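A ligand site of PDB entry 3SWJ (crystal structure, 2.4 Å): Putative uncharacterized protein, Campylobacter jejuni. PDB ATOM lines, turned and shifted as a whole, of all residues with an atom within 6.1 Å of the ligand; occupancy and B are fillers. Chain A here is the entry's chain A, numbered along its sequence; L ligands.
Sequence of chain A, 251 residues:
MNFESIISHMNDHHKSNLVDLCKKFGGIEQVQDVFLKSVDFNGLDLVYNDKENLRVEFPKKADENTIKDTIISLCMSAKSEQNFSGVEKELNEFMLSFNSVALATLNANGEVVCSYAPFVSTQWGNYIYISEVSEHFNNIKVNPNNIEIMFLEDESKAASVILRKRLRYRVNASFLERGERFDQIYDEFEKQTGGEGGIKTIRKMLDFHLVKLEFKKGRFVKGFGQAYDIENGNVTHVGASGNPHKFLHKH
A ring nitrogen (NE2) of His 245 is bound to an iron atom (FE1) of the ligand (2.3 Å). NH1 of Arg 219 is in salt-bridge range of O3 of the ligand, at 2.7 Å. The guanidinium group of Arg 166 lies within salt-bridge range of an oxygen (O4) of the ligand, 2.9 Å away. An oxygen (O3) of the ligand is in salt-bridge range of the guanidinium group (NH1) of Arg 168, 3.7 Å away.
The side-chain amide nitrogen (ND2) of Asn 243 sits at hydrogen-bond distance from the backbone carbonyl oxygen (O) of Lys 24 (2.9 Å). OD1 of Asn 243 sits at hydrogen-bond distance from N of His 245 (2.9 Å). N of Val 238 lies within hydrogen-bond range of O of Ala 227, at 3.4 Å. O of Gly 225 sits at hydrogen-bond distance from NE2 of His 237 (2.9 Å). The backbone carbonyl oxygen (O) of Arg 219 lies within hydrogen-bond range of the backbone NH (N) of Arg 168 (2.9 Å). The backbone carbonyl oxygen of Arg 166 sits at hydrogen-bond distance from the backbone NH of Val 221 (3.1 Å).
Merely in contact with the ligand: Lys 24 (3.6 Å), Phe 25 (3.3 Å), Ile 162 (3.5 Å), Val 221 (3.9 Å), Phe 224 (3.5 Å), Gly 225 (3.4 Å), Ala 227 (3.9 Å), His 237 (3.95 Å), Val 238 (3.5 Å), Gly 239 (3.6 Å), Asn 243 (3.6 Å) and Pro 244 (3.4 Å). Hydrophobic or aromatic side chains within 4 Å of the ligand: Phe 25, Val 221, Phe 224, Ala 227, His 237, Val 238, Pro 244 and His 245. Of the 22 residues printed, 16 come within 4 Å of the ligand. Along chain A the residues within 4 Å of the ligand span positions 24 to 245.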
ATOM      1  N   LYS A  24      -2.313  21.824  11.523  1.00  0.00           N
ATOM      2  CA  LYS A  24      -3.307  21.511  12.539  1.00  0.00           C
ATOM      3  C   LYS A  24      -4.002  22.741  13.126  1.00  0.00           C
ATOM      4  O   LYS A  24      -5.125  22.651  13.628  1.00  0.00           O
ATOM      5  CB  LYS A  24      -2.680  20.646  13.631  1.00  0.00           C
ATOM      6  CG  LYS A  24      -2.806  21.201  15.037  1.00  0.00           C
ATOM      7  CD  LYS A  24      -3.689  20.319  15.914  1.00  0.00           C
ATOM      8  CE  LYS A  24      -3.902  20.949  17.283  1.00  0.00           C
ATOM      9  NZ  LYS A  24      -2.635  20.993  18.069  1.00  0.00           N
ATOM     10  N   PHE A  25      -3.336  23.891  13.083  1.00  0.00           N
ATOM     11  CA  PHE A  25      -3.935  25.139  13.518  1.00  0.00           C
ATOM     12  C   PHE A  25      -4.310  26.000  12.308  1.00  0.00           C
ATOM     13  O   PHE A  25      -4.887  27.079  12.452  1.00  0.00           O
ATOM     14  CB  PHE A  25      -2.984  25.910  14.433  1.00  0.00           C
ATOM     15  CG  PHE A  25      -3.038  25.472  15.870  1.00  0.00           C
ATOM     16  CD1 PHE A  25      -2.291  24.395  16.314  1.00  0.00           C
ATOM     17  CD2 PHE A  25      -3.853  26.132  16.771  1.00  0.00           C
ATOM     18  CE1 PHE A  25      -2.349  23.999  17.632  1.00  0.00           C
ATOM     19  CE2 PHE A  25      -3.921  25.744  18.095  1.00  0.00           C
ATOM     20  CZ  PHE A  25      -3.162  24.670  18.523  1.00  0.00           C
ATOM     21  N   GLY A  26      -3.981  25.494  11.125  1.00  0.00           N
ATOM     22  CA  GLY A  26      -4.321  26.150   9.873  1.00  0.00           C
ATOM     23  C   GLY A  26      -5.003  25.213   8.890  1.00  0.00           C
ATOM     24  O   GLY A  26      -5.732  25.655   8.010  1.00  0.00           O
ATOM     25  N   ILE A 162     -14.062  27.121  26.575  1.00  0.00           N
ATOM     26  CA  ILE A 162     -14.208  26.398  25.322  1.00  0.00           C
ATOM     27  C   ILE A 162     -13.397  25.105  25.300  1.00  0.00           C
ATOM     28  O   ILE A 162     -13.367  24.411  24.286  1.00  0.00           O
ATOM     29  CB  ILE A 162     -13.786  27.243  24.104  1.00  0.00           C
ATOM     30  CG1 ILE A 162     -12.261  27.450  24.097  1.00  0.00           C
ATOM     31  CG2 ILE A 162     -14.539  28.576  24.074  1.00  0.00           C
ATOM     32  CD1 ILE A 162     -11.710  27.813  22.740  1.00  0.00           C
ATOM     33  N   LEU A 163     -12.735  24.799  26.410  1.00  0.00           N
ATOM     34  CA  LEU A 163     -11.966  23.558  26.526  1.00  0.00           C
ATOM     35  C   LEU A 163     -12.036  22.985  27.945  1.00  0.00           C
ATOM     36  O   LEU A 163     -11.005  22.846  28.600  1.00  0.00           O
ATOM     37  CB  LEU A 163     -10.497  23.789  26.139  1.00  0.00           C
ATOM     38  CG  LEU A 163      -9.819  22.678  25.336  1.00  0.00           C
ATOM     39  CD1 LEU A 163      -8.308  22.727  25.543  1.00  0.00           C
ATOM     40  CD2 LEU A 163     -10.363  21.310  25.704  1.00  0.00           C
ATOM     41  N   ARG A 166     -13.685  16.544  29.440  1.00  0.00           N
ATOM     42  CA  ARG A 166     -14.959  15.860  29.615  1.00  0.00           C
ATOM     43  C   ARG A 166     -14.873  14.391  29.231  1.00  0.00           C
ATOM     44  O   ARG A 166     -14.102  14.015  28.340  1.00  0.00           O
ATOM     45  CB  ARG A 166     -16.052  16.566  28.789  1.00  0.00           C
ATOM     46  CG  ARG A 166     -15.999  16.295  27.286  1.00  0.00           C
ATOM     47  CD  ARG A 166     -16.566  17.455  26.476  1.00  0.00           C
ATOM     48  NE  ARG A 166     -15.581  18.509  26.249  1.00  0.00           N
ATOM     49  CZ  ARG A 166     -15.181  18.932  25.052  1.00  0.00           C
ATOM     50  NH1 ARG A 166     -14.267  19.897  24.948  1.00  0.00           N
ATOM     51  NH2 ARG A 166     -15.691  18.392  23.952  1.00  0.00           N
ATOM     52  N   ARG A 168     -17.576  11.103  28.494  1.00  0.00           N
ATOM     53  CA  ARG A 168     -18.989  10.773  28.278  1.00  0.00           C
ATOM     54  C   ARG A 168     -19.218   9.293  27.978  1.00  0.00           C
ATOM     55  O   ARG A 168     -18.602   8.738  27.064  1.00  0.00           O
ATOM     56  CB  ARG A 168     -19.565  11.609  27.145  1.00  0.00           C
ATOM     57  CG  ARG A 168     -19.657  13.112  27.420  1.00  0.00           C
ATOM     58  CD  ARG A 168     -19.831  13.883  26.116  1.00  0.00           C
ATOM     59  NE  ARG A 168     -20.798  13.233  25.232  1.00  0.00           N
ATOM     60  CZ  ARG A 168     -20.658  13.148  23.903  1.00  0.00           C
ATOM     61  NH1 ARG A 168     -19.602  13.671  23.305  1.00  0.00           N
ATOM     62  NH2 ARG A 168     -21.589  12.525  23.184  1.00  0.00           N
ATOM     63  N   ARG A 219     -16.276   8.534  25.260  1.00  0.00           N
ATOM     64  CA  ARG A 219     -15.676   9.630  24.498  1.00  0.00           C
ATOM     65  C   ARG A 219     -14.952  10.542  25.483  1.00  0.00           C
ATOM     66  O   ARG A 219     -15.545  11.026  26.440  1.00  0.00           O
ATOM     67  CB  ARG A 219     -16.748  10.399  23.720  1.00  0.00           C
ATOM     68  CG  ARG A 219     -16.324  11.786  23.221  1.00  0.00           C
ATOM     69  CD  ARG A 219     -15.237  11.711  22.177  1.00  0.00           C
ATOM     70  NE  ARG A 219     -15.642  10.976  20.974  1.00  0.00           N
ATOM     71  CZ  ARG A 219     -16.179  11.549  19.892  1.00  0.00           C
ATOM     72  NH1 ARG A 219     -16.395  12.857  19.867  1.00  0.00           N
ATOM     73  NH2 ARG A 219     -16.507  10.812  18.842  1.00  0.00           N
ATOM     74  N   VAL A 221     -12.305  13.942  25.826  1.00  0.00           N
ATOM     75  CA  VAL A 221     -11.659  15.111  25.218  1.00  0.00           C
ATOM     76  C   VAL A 221     -10.765  15.796  26.240  1.00  0.00           C
ATOM     77  O   VAL A 221     -11.237  16.243  27.289  1.00  0.00           O
ATOM     78  CB  VAL A 221     -12.688  16.125  24.677  1.00  0.00           C
ATOM     79  CG1 VAL A 221     -11.983  17.349  24.094  1.00  0.00           C
ATOM     80  CG2 VAL A 221     -13.597  15.485  23.639  1.00  0.00           C
ATOM     81  N   PHE A 224      -7.466  20.476  22.402  1.00  0.00           N
ATOM     82  CA  PHE A 224      -7.659  20.673  20.966  1.00  0.00           C
ATOM     83  C   PHE A 224      -6.964  19.591  20.154  1.00  0.00           C
ATOM     84  O   PHE A 224      -5.764  19.359  20.311  1.00  0.00           O
ATOM     85  CB  PHE A 224      -7.145  22.049  20.540  1.00  0.00           C
ATOM     86  CG  PHE A 224      -7.821  23.191  21.263  1.00  0.00           C
ATOM     87  CD1 PHE A 224      -9.176  23.156  21.512  1.00  0.00           C
ATOM     88  CD2 PHE A 224      -7.085  24.275  21.703  1.00  0.00           C
ATOM     89  CE1 PHE A 224      -9.810  24.194  22.176  1.00  0.00           C
ATOM     90  CE2 PHE A 224      -7.700  25.323  22.369  1.00  0.00           C
ATOM     91  CZ  PHE A 224      -9.069  25.279  22.607  1.00  0.00           C
ATOM     92  N   GLY A 225      -7.721  18.931  19.281  1.00  0.00           N
ATOM     93  CA  GLY A 225      -7.191  17.841  18.487  1.00  0.00           C
ATOM     94  C   GLY A 225      -6.999  16.571  19.300  1.00  0.00           C
ATOM     95  O   GLY A 225      -6.381  15.607  18.833  1.00  0.00           O
ATOM     96  N   GLN A 226      -7.542  16.555  20.517  1.00  0.00           N
ATOM     97  CA  GLN A 226      -7.354  15.421  21.408  1.00  0.00           C
ATOM     98  C   GLN A 226      -8.661  14.790  21.888  1.00  0.00           C
ATOM     99  O   GLN A 226      -8.978  14.822  23.086  1.00  0.00           O
ATOM    100  CB  GLN A 226      -6.488  15.835  22.606  1.00  0.00           C
ATOM    101  CG  GLN A 226      -5.273  16.663  22.213  1.00  0.00           C
ATOM    102  CD  GLN A 226      -4.068  16.366  23.078  1.00  0.00           C
ATOM    103  OE1 GLN A 226      -3.827  17.033  24.095  1.00  0.00           O
ATOM    104  NE2 GLN A 226      -3.289  15.359  22.693  1.00  0.00           N
ATOM    105  N   ALA A 227      -9.416  14.218  20.943  1.00  0.00           N
ATOM    106  CA  ALA A 227     -10.639  13.486  21.270  1.00  0.00           C
ATOM    107  C   ALA A 227     -10.445  11.986  21.043  1.00  0.00           C
ATOM    108  O   ALA A 227      -9.943  11.566  20.006  1.00  0.00           O
ATOM    109  CB  ALA A 227     -11.816  14.006  20.444  1.00  0.00           C
ATOM    110  N   HIS A 237      -7.932   7.380  18.836  1.00  0.00           N
ATOM    111  CA  HIS A 237      -7.916   8.775  18.396  1.00  0.00           C
ATOM    112  C   HIS A 237      -8.873   8.917  17.214  1.00  0.00           C
ATOM    113  O   HIS A 237      -9.133   7.920  16.519  1.00  0.00           O
ATOM    114  CB  HIS A 237      -6.509   9.259  18.014  1.00  0.00           C
ATOM    115  CG  HIS A 237      -6.344  10.747  18.048  1.00  0.00           C
ATOM    116  ND1 HIS A 237      -7.265  11.605  17.476  1.00  0.00           N
ATOM    117  CD2 HIS A 237      -5.380  11.531  18.580  1.00  0.00           C
ATOM    118  CE1 HIS A 237      -6.864  12.852  17.654  1.00  0.00           C
ATOM    119  NE2 HIS A 237      -5.727  12.832  18.315  1.00  0.00           N
ATOM    120  N   VAL A 238      -9.409  10.112  16.984  1.00  0.00           N
ATOM    121  CA  VAL A 238     -10.592  10.195  16.116  1.00  0.00           C
ATOM    122  C   VAL A 238     -10.447   9.750  14.653  1.00  0.00           C
ATOM    123  O   VAL A 238     -10.944   8.678  14.333  1.00  0.00           O
ATOM    124  CB  VAL A 238     -11.478  11.444  16.338  1.00  0.00           C
ATOM    125  CG1 VAL A 238     -12.384  11.218  17.588  1.00  0.00           C
ATOM    126  CG2 VAL A 238     -10.637  12.652  16.512  1.00  0.00           C
ATOM    127  N   GLY A 239      -9.803  10.502  13.749  1.00  0.00           N
ATOM    128  CA  GLY A 239      -9.228  11.808  13.984  1.00  0.00           C
ATOM    129  C   GLY A 239      -8.152  12.007  12.935  1.00  0.00           C
ATOM    130  O   GLY A 239      -7.943  13.111  12.429  1.00  0.00           O
ATOM    131  N   ALA A 240      -7.444  10.912  12.672  1.00  0.00           N
ATOM    132  CA  ALA A 240      -6.367  10.825  11.706  1.00  0.00           C
ATOM    133  C   ALA A 240      -6.835  11.059  10.266  1.00  0.00           C
ATOM    134  O   ALA A 240      -6.023  11.394   9.408  1.00  0.00           O
ATOM    135  CB  ALA A 240      -5.722   9.458  11.827  1.00  0.00           C
ATOM    136  N   GLY A 242      -7.860  13.443   9.175  1.00  0.00           N
ATOM    137  CA  GLY A 242      -7.696  14.872   8.954  1.00  0.00           C
ATOM    138  C   GLY A 242      -8.372  15.757   9.986  1.00  0.00           C
ATOM    139  O   GLY A 242      -9.324  15.355  10.661  1.00  0.00           O
ATOM    140  N   ASN A 243      -7.843  16.983  10.091  1.00  0.00           N
ATOM    141  CA  ASN A 243      -8.500  18.067  10.818  1.00  0.00           C
ATOM    142  C   ASN A 243      -9.901  18.307  10.262  1.00  0.00           C
ATOM    143  O   ASN A 243     -10.057  18.709   9.103  1.00  0.00           O
ATOM    144  CB  ASN A 243      -7.650  19.335  10.700  1.00  0.00           C
ATOM    145  CG  ASN A 243      -8.120  20.456  11.626  1.00  0.00           C
ATOM    146  OD1 ASN A 243      -9.318  20.634  11.832  1.00  0.00           O
ATOM    147  ND2 ASN A 243      -7.177  21.220  12.165  1.00  0.00           N
ATOM    148  N   PRO A 244     -10.930  18.075  11.081  1.00  0.00           N
ATOM    149  CA  PRO A 244     -12.315  18.137  10.609  1.00  0.00           C
ATOM    150  C   PRO A 244     -12.899  19.555  10.550  1.00  0.00           C
ATOM    151  O   PRO A 244     -14.013  19.734  10.076  1.00  0.00           O
ATOM    152  CB  PRO A 244     -13.074  17.326  11.669  1.00  0.00           C
ATOM    153  CG  PRO A 244     -12.303  17.628  12.932  1.00  0.00           C
ATOM    154  CD  PRO A 244     -10.851  17.722  12.513  1.00  0.00           C
ATOM    155  N   HIS A 245     -12.145  20.542  11.025  1.00  0.00           N
ATOM    156  CA  HIS A 245     -12.638  21.914  11.085  1.00  0.00           C
ATOM    157  C   HIS A 245     -12.419  22.654   9.758  1.00  0.00           C
ATOM    158  O   HIS A 245     -11.633  22.226   8.908  1.00  0.00           O
ATOM    159  CB  HIS A 245     -12.008  22.662  12.264  1.00  0.00           C
ATOM    160  CG  HIS A 245     -12.400  22.090  13.604  1.00  0.00           C
ATOM    161  ND1 HIS A 245     -13.687  21.972  14.012  1.00  0.00           N
ATOM    162  CD2 HIS A 245     -11.605  21.617  14.624  1.00  0.00           C
ATOM    163  CE1 HIS A 245     -13.714  21.429  15.244  1.00  0.00           C
ATOM    164  NE2 HIS A 245     -12.482  21.219  15.612  1.00  0.00           N
ATOM    165  N   PHE A 247     -11.419  26.342   8.223  1.00  0.00           N
ATOM    166  CA  PHE A 247     -10.921  27.710   8.327  1.00  0.00           C
ATOM    167  C   PHE A 247     -11.208  28.441   7.037  1.00  0.00           C
ATOM    168  O   PHE A 247     -11.481  27.823   6.005  1.00  0.00           O
ATOM    169  CB  PHE A 247      -9.412  27.710   8.575  1.00  0.00           C
ATOM    170  CG  PHE A 247      -8.967  26.739   9.622  1.00  0.00           C
ATOM    171  CD1 PHE A 247      -8.722  27.170  10.927  1.00  0.00           C
ATOM    172  CD2 PHE A 247      -8.810  25.396   9.317  1.00  0.00           C
ATOM    173  CE1 PHE A 247      -8.314  26.267  11.895  1.00  0.00           C
ATOM    174  CE2 PHE A 247      -8.402  24.493  10.286  1.00  0.00           C
ATOM    175  CZ  PHE A 247      -8.159  24.921  11.577  1.00  0.00           C
HETATM  176  C1  LIG L   1     -14.630  19.504  18.815  1.00  0.00           C
HETATM  177  C2  LIG L   1     -11.642  23.357  19.033  1.00  0.00           C
HETATM  178  C3  LIG L   1      -8.390  21.052  16.211  1.00  0.00           C
HETATM  179  C4  LIG L   1     -11.265  17.137  16.150  1.00  0.00           C
HETATM  180  C5  LIG L   1     -14.101  20.736  19.130  1.00  0.00           C
HETATM  181  C6  LIG L   1     -14.716  21.732  19.998  1.00  0.00           C
HETATM  182  C7  LIG L   1     -13.891  22.797  20.054  1.00  0.00           C
HETATM  183  C8  LIG L   1     -12.727  22.520  19.233  1.00  0.00           C
HETATM  184  C9  LIG L   1     -14.132  24.093  20.859  1.00  0.00           C
HETATM  185  C10 LIG L   1     -16.079  21.595  20.732  1.00  0.00           C
HETATM  186  C11 LIG L   1     -17.222  21.844  19.755  1.00  0.00           C
HETATM  187  C12 LIG L   1     -18.562  21.465  20.346  1.00  0.00           C
HETATM  188  O1  LIG L   1     -18.612  20.866  21.455  1.00  0.00           O
HETATM  189  O2  LIG L   1     -19.603  21.766  19.682  1.00  0.00           O
HETATM  190  C13 LIG L   1     -10.507  23.090  18.278  1.00  0.00           C
HETATM  191  C14 LIG L   1      -9.390  23.985  18.010  1.00  0.00           C
HETATM  192  C15 LIG L   1      -8.497  23.323  17.263  1.00  0.00           C
HETATM  193  C16 LIG L   1      -9.029  22.007  16.982  1.00  0.00           C
HETATM  194  C17 LIG L   1      -9.226  25.433  18.543  1.00  0.00           C
HETATM  195  C18 LIG L   1      -7.154  23.830  16.692  1.00  0.00           C
HETATM  196  C19 LIG L   1      -6.971  25.116  16.378  1.00  0.00           C
HETATM  197  C20 LIG L   1      -8.847  19.771  15.989  1.00  0.00           C
HETATM  198  C21 LIG L   1      -8.133  18.683  15.337  1.00  0.00           C
HETATM  199  C22 LIG L   1      -8.955  17.625  15.308  1.00  0.00           C
HETATM  200  C23 LIG L   1     -10.189  17.985  15.970  1.00  0.00           C
HETATM  201  C24 LIG L   1      -6.707  18.753  14.737  1.00  0.00           C
HETATM  202  C25 LIG L   1      -8.672  16.206  14.761  1.00  0.00           C
HETATM  203  C26 LIG L   1      -7.474  15.637  14.918  1.00  0.00           C
HETATM  204  C27 LIG L   1     -12.390  17.364  16.906  1.00  0.00           C
HETATM  205  C28 LIG L   1     -13.347  16.352  17.281  1.00  0.00           C
HETATM  206  C29 LIG L   1     -14.406  17.075  18.118  1.00  0.00           C
HETATM  207  C30 LIG L   1     -13.977  18.466  18.164  1.00  0.00           C
HETATM  208  C31 LIG L   1     -13.326  14.844  16.919  1.00  0.00           C
HETATM  209  C32 LIG L   1     -15.657  16.448  18.774  1.00  0.00           C
HETATM  210  C33 LIG L   1     -15.422  16.328  20.275  1.00  0.00           C
HETATM  211  C34 LIG L   1     -16.740  16.151  20.984  1.00  0.00           C
HETATM  212  O3  LIG L   1     -17.452  15.152  20.698  1.00  0.00           O
HETATM  213  O4  LIG L   1     -17.072  16.999  21.846  1.00  0.00           O
HETATM  214  N1  LIG L   1     -12.896  21.258  18.686  1.00  0.00           N
HETATM  215  N2  LIG L   1     -10.243  21.901  17.628  1.00  0.00           N
HETATM  216  N3  LIG L   1     -10.089  19.295  16.352  1.00  0.00           N
HETATM  217  N4  LIG L   1     -12.787  18.591  17.443  1.00  0.00           N
HETATM  218 FE1  LIG L   1     -11.502  20.278  17.432  1.00  0.00          FE
